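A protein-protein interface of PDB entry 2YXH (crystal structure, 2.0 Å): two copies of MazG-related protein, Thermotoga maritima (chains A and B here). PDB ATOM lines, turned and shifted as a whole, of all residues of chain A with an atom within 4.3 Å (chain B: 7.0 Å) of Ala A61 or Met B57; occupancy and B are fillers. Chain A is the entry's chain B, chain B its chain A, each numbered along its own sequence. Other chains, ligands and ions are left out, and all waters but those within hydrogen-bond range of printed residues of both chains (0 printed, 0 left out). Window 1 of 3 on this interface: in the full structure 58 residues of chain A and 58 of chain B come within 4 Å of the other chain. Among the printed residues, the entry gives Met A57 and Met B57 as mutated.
Among the printed residues, merely in contact across the chains: Leu A31 with Ile B35 (3.97 Å), Leu A31 with Met B57 (3.7 Å), Met A57 with Leu B31 (3.8 Å), Met A57 with Ala B61 (3.4 Å), Ala A61 with Met B57 (3.3 Å), Val A64 with Ile B54 (3.9 Å) and Val A64 with Met B57 (3.7 Å).
Printed residues of chain B within 4 Å of Leu A31: Ile B35 and Met B57.
Of the printed residues of chain B, Ala A61 touches Met B57.
Ala A65 touches none of the printed residues of chain B.
Met B57 touches just these residues of chain A: Leu A31, Ala A61 and Val A64.
Of the printed residues of chain A, Ala B61 touches Met A57.
Leu A31 touches Met B57, and with the chains exchanged Met A57 touches Leu B31.
Met A57 touches Ala B61, and with the chains exchanged Ala A61 touches Met B57.
Positions printed for both chains: 31, 57, 58, 59, 60, 61, 62 and 63.
Of the 7 pairs that touch across the chains among the printed residues, 4 have their exchanged pair printed and touching as well.
Of the 10 printed residues of chain A, 4 touch a printed residue of chain B.
Of the 16 printed residues of chain B, 5 touch a printed residue of chain A.
Hydrophobic or aromatic side chains of chain B within 4 Å of the printed part of chain A: Leu B31, Ile B35, Ile B54 and Met B57.
Along chain B the printed residues that touch a printed residue of chain A span positions 31 to 61.
Among the printed residues, 7 pairs touch across the chains.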
ATOM      1  N   LEU A  31      -9.957   3.972  -1.190  1.00  0.00           N
ATOM      2  CA  LEU A  31     -11.024   3.055  -1.602  1.00  0.00           C
ATOM      3  C   LEU A  31     -10.334   1.757  -2.035  1.00  0.00           C
ATOM      4  O   LEU A  31     -10.747   0.675  -1.681  1.00  0.00           O
ATOM      5  CB  LEU A  31     -11.734   3.607  -2.821  1.00  0.00           C
ATOM      6  CG  LEU A  31     -12.839   2.751  -3.468  1.00  0.00           C
ATOM      7  CD1 LEU A  31     -13.773   2.103  -2.428  1.00  0.00           C
ATOM      8  CD2 LEU A  31     -13.650   3.638  -4.480  1.00  0.00           C
ATOM      9  N   MET A  57     -16.259   0.260   2.392  1.00  0.00           N
ATOM     10  CA  MET A  57     -16.097   0.410   0.937  1.00  0.00           C
ATOM     11  C   MET A  57     -17.179   1.376   0.392  1.00  0.00           C
ATOM     12  O   MET A  57     -16.831   2.319  -0.287  1.00  0.00           O
ATOM     13  CB  MET A  57     -16.096  -0.957   0.256  1.00  0.00           C
ATOM     14  CG  MET A  57     -15.836  -0.916  -1.254  1.00  0.00           C
ATOM     15  SD  MET A  57     -16.632  -2.598  -2.067  1.00  0.00           S
ATOM     16  CE  MET A  57     -18.508  -2.557  -1.435  1.00  0.00           C
ATOM     17  N   ILE A  58     -18.466   1.156   0.719  1.00  0.00           N
ATOM     18  CA  ILE A  58     -19.530   2.103   0.300  1.00  0.00           C
ATOM     19  C   ILE A  58     -19.229   3.531   0.771  1.00  0.00           C
ATOM     20  O   ILE A  58     -19.268   4.460  -0.031  1.00  0.00           O
ATOM     21  CB  ILE A  58     -20.901   1.666   0.668  1.00  0.00           C
ATOM     22  CG1 ILE A  58     -21.274   0.480  -0.213  1.00  0.00           C
ATOM     23  CG2 ILE A  58     -21.990   2.813   0.371  1.00  0.00           C
ATOM     24  CD1 ILE A  58     -22.124  -0.495   0.430  1.00  0.00           C
ATOM     25  N   TYR A  59     -18.865   3.700   2.033  1.00  0.00           N
ATOM     26  CA  TYR A  59     -18.488   5.030   2.503  1.00  0.00           C
ATOM     27  C   TYR A  59     -17.305   5.631   1.723  1.00  0.00           C
ATOM     28  O   TYR A  59     -17.350   6.756   1.227  1.00  0.00           O
ATOM     29  CB  TYR A  59     -18.144   4.880   3.955  1.00  0.00           C
ATOM     30  CG  TYR A  59     -17.424   5.996   4.616  1.00  0.00           C
ATOM     31  CD1 TYR A  59     -17.984   7.273   4.711  1.00  0.00           C
ATOM     32  CD2 TYR A  59     -16.279   5.763   5.266  1.00  0.00           C
ATOM     33  CE1 TYR A  59     -17.372   8.283   5.417  1.00  0.00           C
ATOM     34  CE2 TYR A  59     -15.641   6.784   5.934  1.00  0.00           C
ATOM     35  CZ  TYR A  59     -16.223   8.041   6.014  1.00  0.00           C
ATOM     36  OH  TYR A  59     -15.550   9.043   6.693  1.00  0.00           O
ATOM     37  N   ASP A  60     -16.213   4.906   1.645  1.00  0.00           N
ATOM     38  CA  ASP A  60     -15.120   5.481   0.952  1.00  0.00           C
ATOM     39  C   ASP A  60     -15.440   5.774  -0.510  1.00  0.00           C
ATOM     40  O   ASP A  60     -15.105   6.833  -0.952  1.00  0.00           O
ATOM     41  CB  ASP A  60     -13.942   4.539   0.997  1.00  0.00           C
ATOM     42  CG  ASP A  60     -13.162   4.618   2.331  1.00  0.00           C
ATOM     43  OD1 ASP A  60     -13.612   5.348   3.267  1.00  0.00           O
ATOM     44  OD2 ASP A  60     -12.035   3.972   2.396  1.00  0.00           O
ATOM     45  N   ALA A  61     -16.004   4.831  -1.271  1.00  0.00           N
ATOM     46  CA  ALA A  61     -16.523   5.140  -2.611  1.00  0.00           C
ATOM     47  C   ALA A  61     -17.302   6.467  -2.616  1.00  0.00           C
ATOM     48  O   ALA A  61     -17.118   7.302  -3.513  1.00  0.00           O
ATOM     49  CB  ALA A  61     -17.467   3.980  -3.210  1.00  0.00           C
ATOM     50  N   LEU A  62     -18.183   6.662  -1.631  1.00  0.00           N
ATOM     51  CA  LEU A  62     -19.035   7.829  -1.668  1.00  0.00           C
ATOM     52  C   LEU A  62     -18.230   9.054  -1.312  1.00  0.00           C
ATOM     53  O   LEU A  62     -18.584  10.147  -1.787  1.00  0.00           O
ATOM     54  CB  LEU A  62     -20.224   7.722  -0.742  1.00  0.00           C
ATOM     55  CG  LEU A  62     -21.365   6.877  -1.286  1.00  0.00           C
ATOM     56  CD1 LEU A  62     -22.382   6.595  -0.161  1.00  0.00           C
ATOM     57  CD2 LEU A  62     -21.917   7.636  -2.420  1.00  0.00           C
ATOM     58  N   LEU A  63     -17.174   8.889  -0.508  1.00  0.00           N
ATOM     59  CA  LEU A  63     -16.280  10.069  -0.290  1.00  0.00           C
ATOM     60  C   LEU A  63     -15.473  10.485  -1.564  1.00  0.00           C
ATOM     61  O   LEU A  63     -15.176  11.638  -1.746  1.00  0.00           O
ATOM     62  CB  LEU A  63     -15.319   9.871   0.807  1.00  0.00           C
ATOM     63  CG  LEU A  63     -15.649   9.846   2.249  1.00  0.00           C
ATOM     64  CD1 LEU A  63     -14.393   9.342   3.075  1.00  0.00           C
ATOM     65  CD2 LEU A  63     -16.137  11.239   2.653  1.00  0.00           C
ATOM     66  N   VAL A  64     -15.155   9.531  -2.432  1.00  0.00           N
ATOM     67  CA  VAL A  64     -14.553   9.875  -3.744  1.00  0.00           C
ATOM     68  C   VAL A  64     -15.612  10.668  -4.504  1.00  0.00           C
ATOM     69  O   VAL A  64     -15.293  11.716  -5.088  1.00  0.00           O
ATOM     70  CB  VAL A  64     -14.160   8.665  -4.522  1.00  0.00           C
ATOM     71  CG1 VAL A  64     -13.696   9.039  -5.963  1.00  0.00           C
ATOM     72  CG2 VAL A  64     -13.024   7.925  -3.833  1.00  0.00           C
ATOM     73  N   ALA A  65     -16.884  10.242  -4.444  1.00  0.00           N
ATOM     74  CA  ALA A  65     -17.930  10.976  -5.158  1.00  0.00           C
ATOM     75  C   ALA A  65     -17.986  12.414  -4.592  1.00  0.00           C
ATOM     76  O   ALA A  65     -18.071  13.405  -5.318  1.00  0.00           O
ATOM     77  CB  ALA A  65     -19.321  10.248  -4.961  1.00  0.00           C
ATOM     78  N   LEU B  31     -14.291  -3.352  -9.806  1.00  0.00           N
ATOM     79  CA  LEU B  31     -14.264  -2.088  -9.047  1.00  0.00           C
ATOM     80  C   LEU B  31     -12.894  -1.403  -9.023  1.00  0.00           C
ATOM     81  O   LEU B  31     -12.847  -0.181  -9.164  1.00  0.00           O
ATOM     82  CB  LEU B  31     -14.777  -2.278  -7.598  1.00  0.00           C
ATOM     83  CG  LEU B  31     -14.765  -1.032  -6.726  1.00  0.00           C
ATOM     84  CD1 LEU B  31     -15.450   0.191  -7.351  1.00  0.00           C
ATOM     85  CD2 LEU B  31     -15.303  -1.388  -5.410  1.00  0.00           C
ATOM     86  N   GLU B  34     -12.572   0.468 -12.272  1.00  0.00           N
ATOM     87  CA  GLU B  34     -13.204   1.743 -12.480  1.00  0.00           C
ATOM     88  C   GLU B  34     -12.495   2.828 -11.727  1.00  0.00           C
ATOM     89  O   GLU B  34     -12.578   3.972 -12.110  1.00  0.00           O
ATOM     90  CB  GLU B  34     -14.669   1.782 -11.956  1.00  0.00           C
ATOM     91  CG  GLU B  34     -15.534   0.818 -12.559  1.00  0.00           C
ATOM     92  CD  GLU B  34     -15.839   1.150 -14.011  1.00  0.00           C
ATOM     93  OE1 GLU B  34     -15.572   2.308 -14.435  1.00  0.00           O
ATOM     94  OE2 GLU B  34     -16.405   0.268 -14.715  1.00  0.00           O
ATOM     95  N   ILE B  35     -11.978   2.488 -10.562  1.00  0.00           N
ATOM     96  CA  ILE B  35     -11.117   3.368  -9.805  1.00  0.00           C
ATOM     97  C   ILE B  35     -10.010   3.904 -10.739  1.00  0.00           C
ATOM     98  O   ILE B  35      -9.661   5.079 -10.691  1.00  0.00           O
ATOM     99  CB  ILE B  35     -10.371   2.563  -8.695  1.00  0.00           C
ATOM    100  CG1 ILE B  35     -11.202   2.409  -7.469  1.00  0.00           C
ATOM    101  CG2 ILE B  35      -9.012   3.256  -8.289  1.00  0.00           C
ATOM    102  CD1 ILE B  35     -10.490   1.597  -6.449  1.00  0.00           C
ATOM    103  N   VAL B  38     -11.301   6.458 -13.019  1.00  0.00           N
ATOM    104  CA  VAL B  38     -11.631   7.723 -12.361  1.00  0.00           C
ATOM    105  C   VAL B  38     -10.298   8.541 -12.262  1.00  0.00           C
ATOM    106  O   VAL B  38     -10.212   9.741 -12.634  1.00  0.00           O
ATOM    107  CB  VAL B  38     -12.264   7.486 -10.948  1.00  0.00           C
ATOM    108  CG1 VAL B  38     -12.204   8.712 -10.154  1.00  0.00           C
ATOM    109  CG2 VAL B  38     -13.733   7.032 -11.098  1.00  0.00           C
ATOM    110  N   GLU B  52     -19.164  10.222 -15.804  1.00  0.00           N
ATOM    111  CA  GLU B  52     -19.297   8.864 -16.121  1.00  0.00           C
ATOM    112  C   GLU B  52     -18.613   7.883 -15.165  1.00  0.00           C
ATOM    113  O   GLU B  52     -19.249   6.997 -14.687  1.00  0.00           O
ATOM    114  CB  GLU B  52     -18.887   8.610 -17.568  1.00  0.00           C
ATOM    115  CG  GLU B  52     -19.253   7.121 -18.104  1.00  0.00           C
ATOM    116  CD  GLU B  52     -18.231   6.517 -19.164  1.00  0.00           C
ATOM    117  OE1 GLU B  52     -17.546   7.301 -19.870  1.00  0.00           O
ATOM    118  OE2 GLU B  52     -18.167   5.263 -19.305  1.00  0.00           O
ATOM    119  N   GLU B  53     -17.292   7.940 -14.989  1.00  0.00           N
ATOM    120  CA  GLU B  53     -16.662   6.996 -14.160  1.00  0.00           C
ATOM    121  C   GLU B  53     -17.137   7.048 -12.668  1.00  0.00           C
ATOM    122  O   GLU B  53     -17.136   6.018 -11.978  1.00  0.00           O
ATOM    123  CB  GLU B  53     -15.155   7.233 -14.268  1.00  0.00           C
ATOM    124  CG  GLU B  53     -14.743   7.342 -15.781  1.00  0.00           C
ATOM    125  CD  GLU B  53     -15.062   6.039 -16.543  1.00  0.00           C
ATOM    126  OE1 GLU B  53     -15.353   5.000 -15.906  1.00  0.00           O
ATOM    127  OE2 GLU B  53     -15.066   6.028 -17.790  1.00  0.00           O
ATOM    128  N   ILE B  54     -17.397   8.241 -12.145  1.00  0.00           N
ATOM    129  CA  ILE B  54     -17.977   8.288 -10.767  1.00  0.00           C
ATOM    130  C   ILE B  54     -19.227   7.360 -10.713  1.00  0.00           C
ATOM    131  O   ILE B  54     -19.380   6.494  -9.835  1.00  0.00           O
ATOM    132  CB  ILE B  54     -18.280   9.721 -10.319  1.00  0.00           C
ATOM    133  CG1 ILE B  54     -16.916  10.470 -10.113  1.00  0.00           C
ATOM    134  CG2 ILE B  54     -19.019   9.688  -8.947  1.00  0.00           C
ATOM    135  CD1 ILE B  54     -15.996   9.847  -9.031  1.00  0.00           C
ATOM    136  N   GLY B  55     -20.102   7.511 -11.715  1.00  0.00           N
ATOM    137  CA  GLY B  55     -21.253   6.637 -11.720  1.00  0.00           C
ATOM    138  C   GLY B  55     -20.877   5.155 -11.853  1.00  0.00           C
ATOM    139  O   GLY B  55     -21.357   4.309 -11.078  1.00  0.00           O
ATOM    140  N   ASP B  56     -20.023   4.829 -12.834  1.00  0.00           N
ATOM    141  CA  ASP B  56     -19.530   3.455 -12.964  1.00  0.00           C
ATOM    142  C   ASP B  56     -19.029   2.904 -11.657  1.00  0.00           C
ATOM    143  O   ASP B  56     -19.218   1.766 -11.326  1.00  0.00           O
ATOM    144  CB  ASP B  56     -18.385   3.462 -13.942  1.00  0.00           C
ATOM    145  CG  ASP B  56     -18.836   3.519 -15.359  1.00  0.00           C
ATOM    146  OD1 ASP B  56     -20.044   3.574 -15.670  1.00  0.00           O
ATOM    147  OD2 ASP B  56     -18.020   3.391 -16.205  1.00  0.00           O
ATOM    148  N   MET B  57     -18.300   3.736 -10.935  1.00  0.00           N
ATOM    149  CA  MET B  57     -17.592   3.349  -9.746  1.00  0.00           C
ATOM    150  C   MET B  57     -18.570   2.995  -8.635  1.00  0.00           C
ATOM    151  O   MET B  57     -18.405   2.011  -7.942  1.00  0.00           O
ATOM    152  CB  MET B  57     -16.712   4.542  -9.312  1.00  0.00           C
ATOM    153  CG  MET B  57     -15.966   4.219  -7.967  1.00  0.00           C
ATOM    154  SD  MET B  57     -15.183   5.780  -7.040  1.00  0.00           S
ATOM    155  CE  MET B  57     -16.926   6.831  -6.746  1.00  0.00           C
ATOM    156  N   ILE B  58     -19.581   3.847  -8.453  1.00  0.00           N
ATOM    157  CA  ILE B  58     -20.593   3.616  -7.428  1.00  0.00           C
ATOM    158  C   ILE B  58     -21.456   2.352  -7.714  1.00  0.00           C
ATOM    159  O   ILE B  58     -21.704   1.523  -6.808  1.00  0.00           O
ATOM    160  CB  ILE B  58     -21.540   4.805  -7.309  1.00  0.00           C
ATOM    161  CG1 ILE B  58     -20.842   5.968  -6.596  1.00  0.00           C
ATOM    162  CG2 ILE B  58     -22.854   4.361  -6.569  1.00  0.00           C
ATOM    163  CD1 ILE B  58     -21.725   7.241  -6.547  1.00  0.00           C
ATOM    164  N   TYR B  59     -21.889   2.215  -8.969  1.00  0.00           N
ATOM    165  CA  TYR B  59     -22.517   0.988  -9.418  1.00  0.00           C
ATOM    166  C   TYR B  59     -21.675  -0.268  -9.106  1.00  0.00           C
ATOM    167  O   TYR B  59     -22.178  -1.283  -8.571  1.00  0.00           O
ATOM    168  CB  TYR B  59     -22.765   1.122 -10.892  1.00  0.00           C
ATOM    169  CG  TYR B  59     -23.217  -0.094 -11.586  1.00  0.00           C
ATOM    170  CD1 TYR B  59     -24.440  -0.694 -11.258  1.00  0.00           C
ATOM    171  CD2 TYR B  59     -22.443  -0.658 -12.622  1.00  0.00           C
ATOM    172  CE1 TYR B  59     -24.905  -1.855 -11.949  1.00  0.00           C
ATOM    173  CE2 TYR B  59     -22.897  -1.886 -13.334  1.00  0.00           C
ATOM    174  CZ  TYR B  59     -24.141  -2.417 -12.978  1.00  0.00           C
ATOM    175  OH  TYR B  59     -24.646  -3.546 -13.598  1.00  0.00           O
ATOM    176  N   ASP B  60     -20.412  -0.233  -9.482  1.00  0.00           N
ATOM    177  CA  ASP B  60     -19.601  -1.392  -9.251  1.00  0.00           C
ATOM    178  C   ASP B  60     -19.375  -1.717  -7.802  1.00  0.00           C
ATOM    179  O   ASP B  60     -19.370  -2.871  -7.441  1.00  0.00           O
ATOM    180  CB  ASP B  60     -18.286  -1.228  -9.963  1.00  0.00           C
ATOM    181  CG  ASP B  60     -18.405  -1.543 -11.496  1.00  0.00           C
ATOM    182  OD1 ASP B  60     -19.517  -1.854 -12.048  1.00  0.00           O
ATOM    183  OD2 ASP B  60     -17.379  -1.471 -12.162  1.00  0.00           O
ATOM    184  N   ALA B  61     -19.192  -0.718  -6.948  1.00  0.00           N
ATOM    185  CA  ALA B  61     -19.104  -0.955  -5.525  1.00  0.00           C
ATOM    186  C   ALA B  61     -20.428  -1.586  -5.057  1.00  0.00           C
ATOM    187  O   ALA B  61     -20.491  -2.490  -4.213  1.00  0.00           O
ATOM    188  CB  ALA B  61     -18.938   0.313  -4.820  1.00  0.00           C
ATOM    189  N   LEU B  62     -21.514  -1.044  -5.558  1.00  0.00           N
ATOM    190  CA  LEU B  62     -22.800  -1.572  -5.133  1.00  0.00           C
ATOM    191  C   LEU B  62     -23.010  -2.977  -5.635  1.00  0.00           C
ATOM    192  O   LEU B  62     -23.540  -3.779  -4.883  1.00  0.00           O
ATOM    193  CB  LEU B  62     -23.900  -0.623  -5.566  1.00  0.00           C
ATOM    194  CG  LEU B  62     -24.103   0.619  -4.704  1.00  0.00           C
ATOM    195  CD1 LEU B  62     -25.357   1.333  -5.344  1.00  0.00           C
ATOM    196  CD2 LEU B  62     -24.462   0.197  -3.251  1.00  0.00           C
ATOM    197  N   LEU B  63     -22.471  -3.342  -6.816  1.00  0.00           N
ATOM    198  CA  LEU B  63     -22.499  -4.742  -7.223  1.00  0.00           C
ATOM    199  C   LEU B  63     -21.607  -5.623  -6.326  1.00  0.00           C
ATOM    200  O   LEU B  63     -21.888  -6.788  -6.133  1.00  0.00           O
ATOM    201  CB  LEU B  63     -22.056  -4.968  -8.620  1.00  0.00           C
ATOM    202  CG  LEU B  63     -23.017  -4.720  -9.755  1.00  0.00           C
ATOM    203  CD1 LEU B  63     -22.230  -4.953 -11.105  1.00  0.00           C
ATOM    204  CD2 LEU B  63     -24.462  -5.473  -9.622  1.00  0.00           C
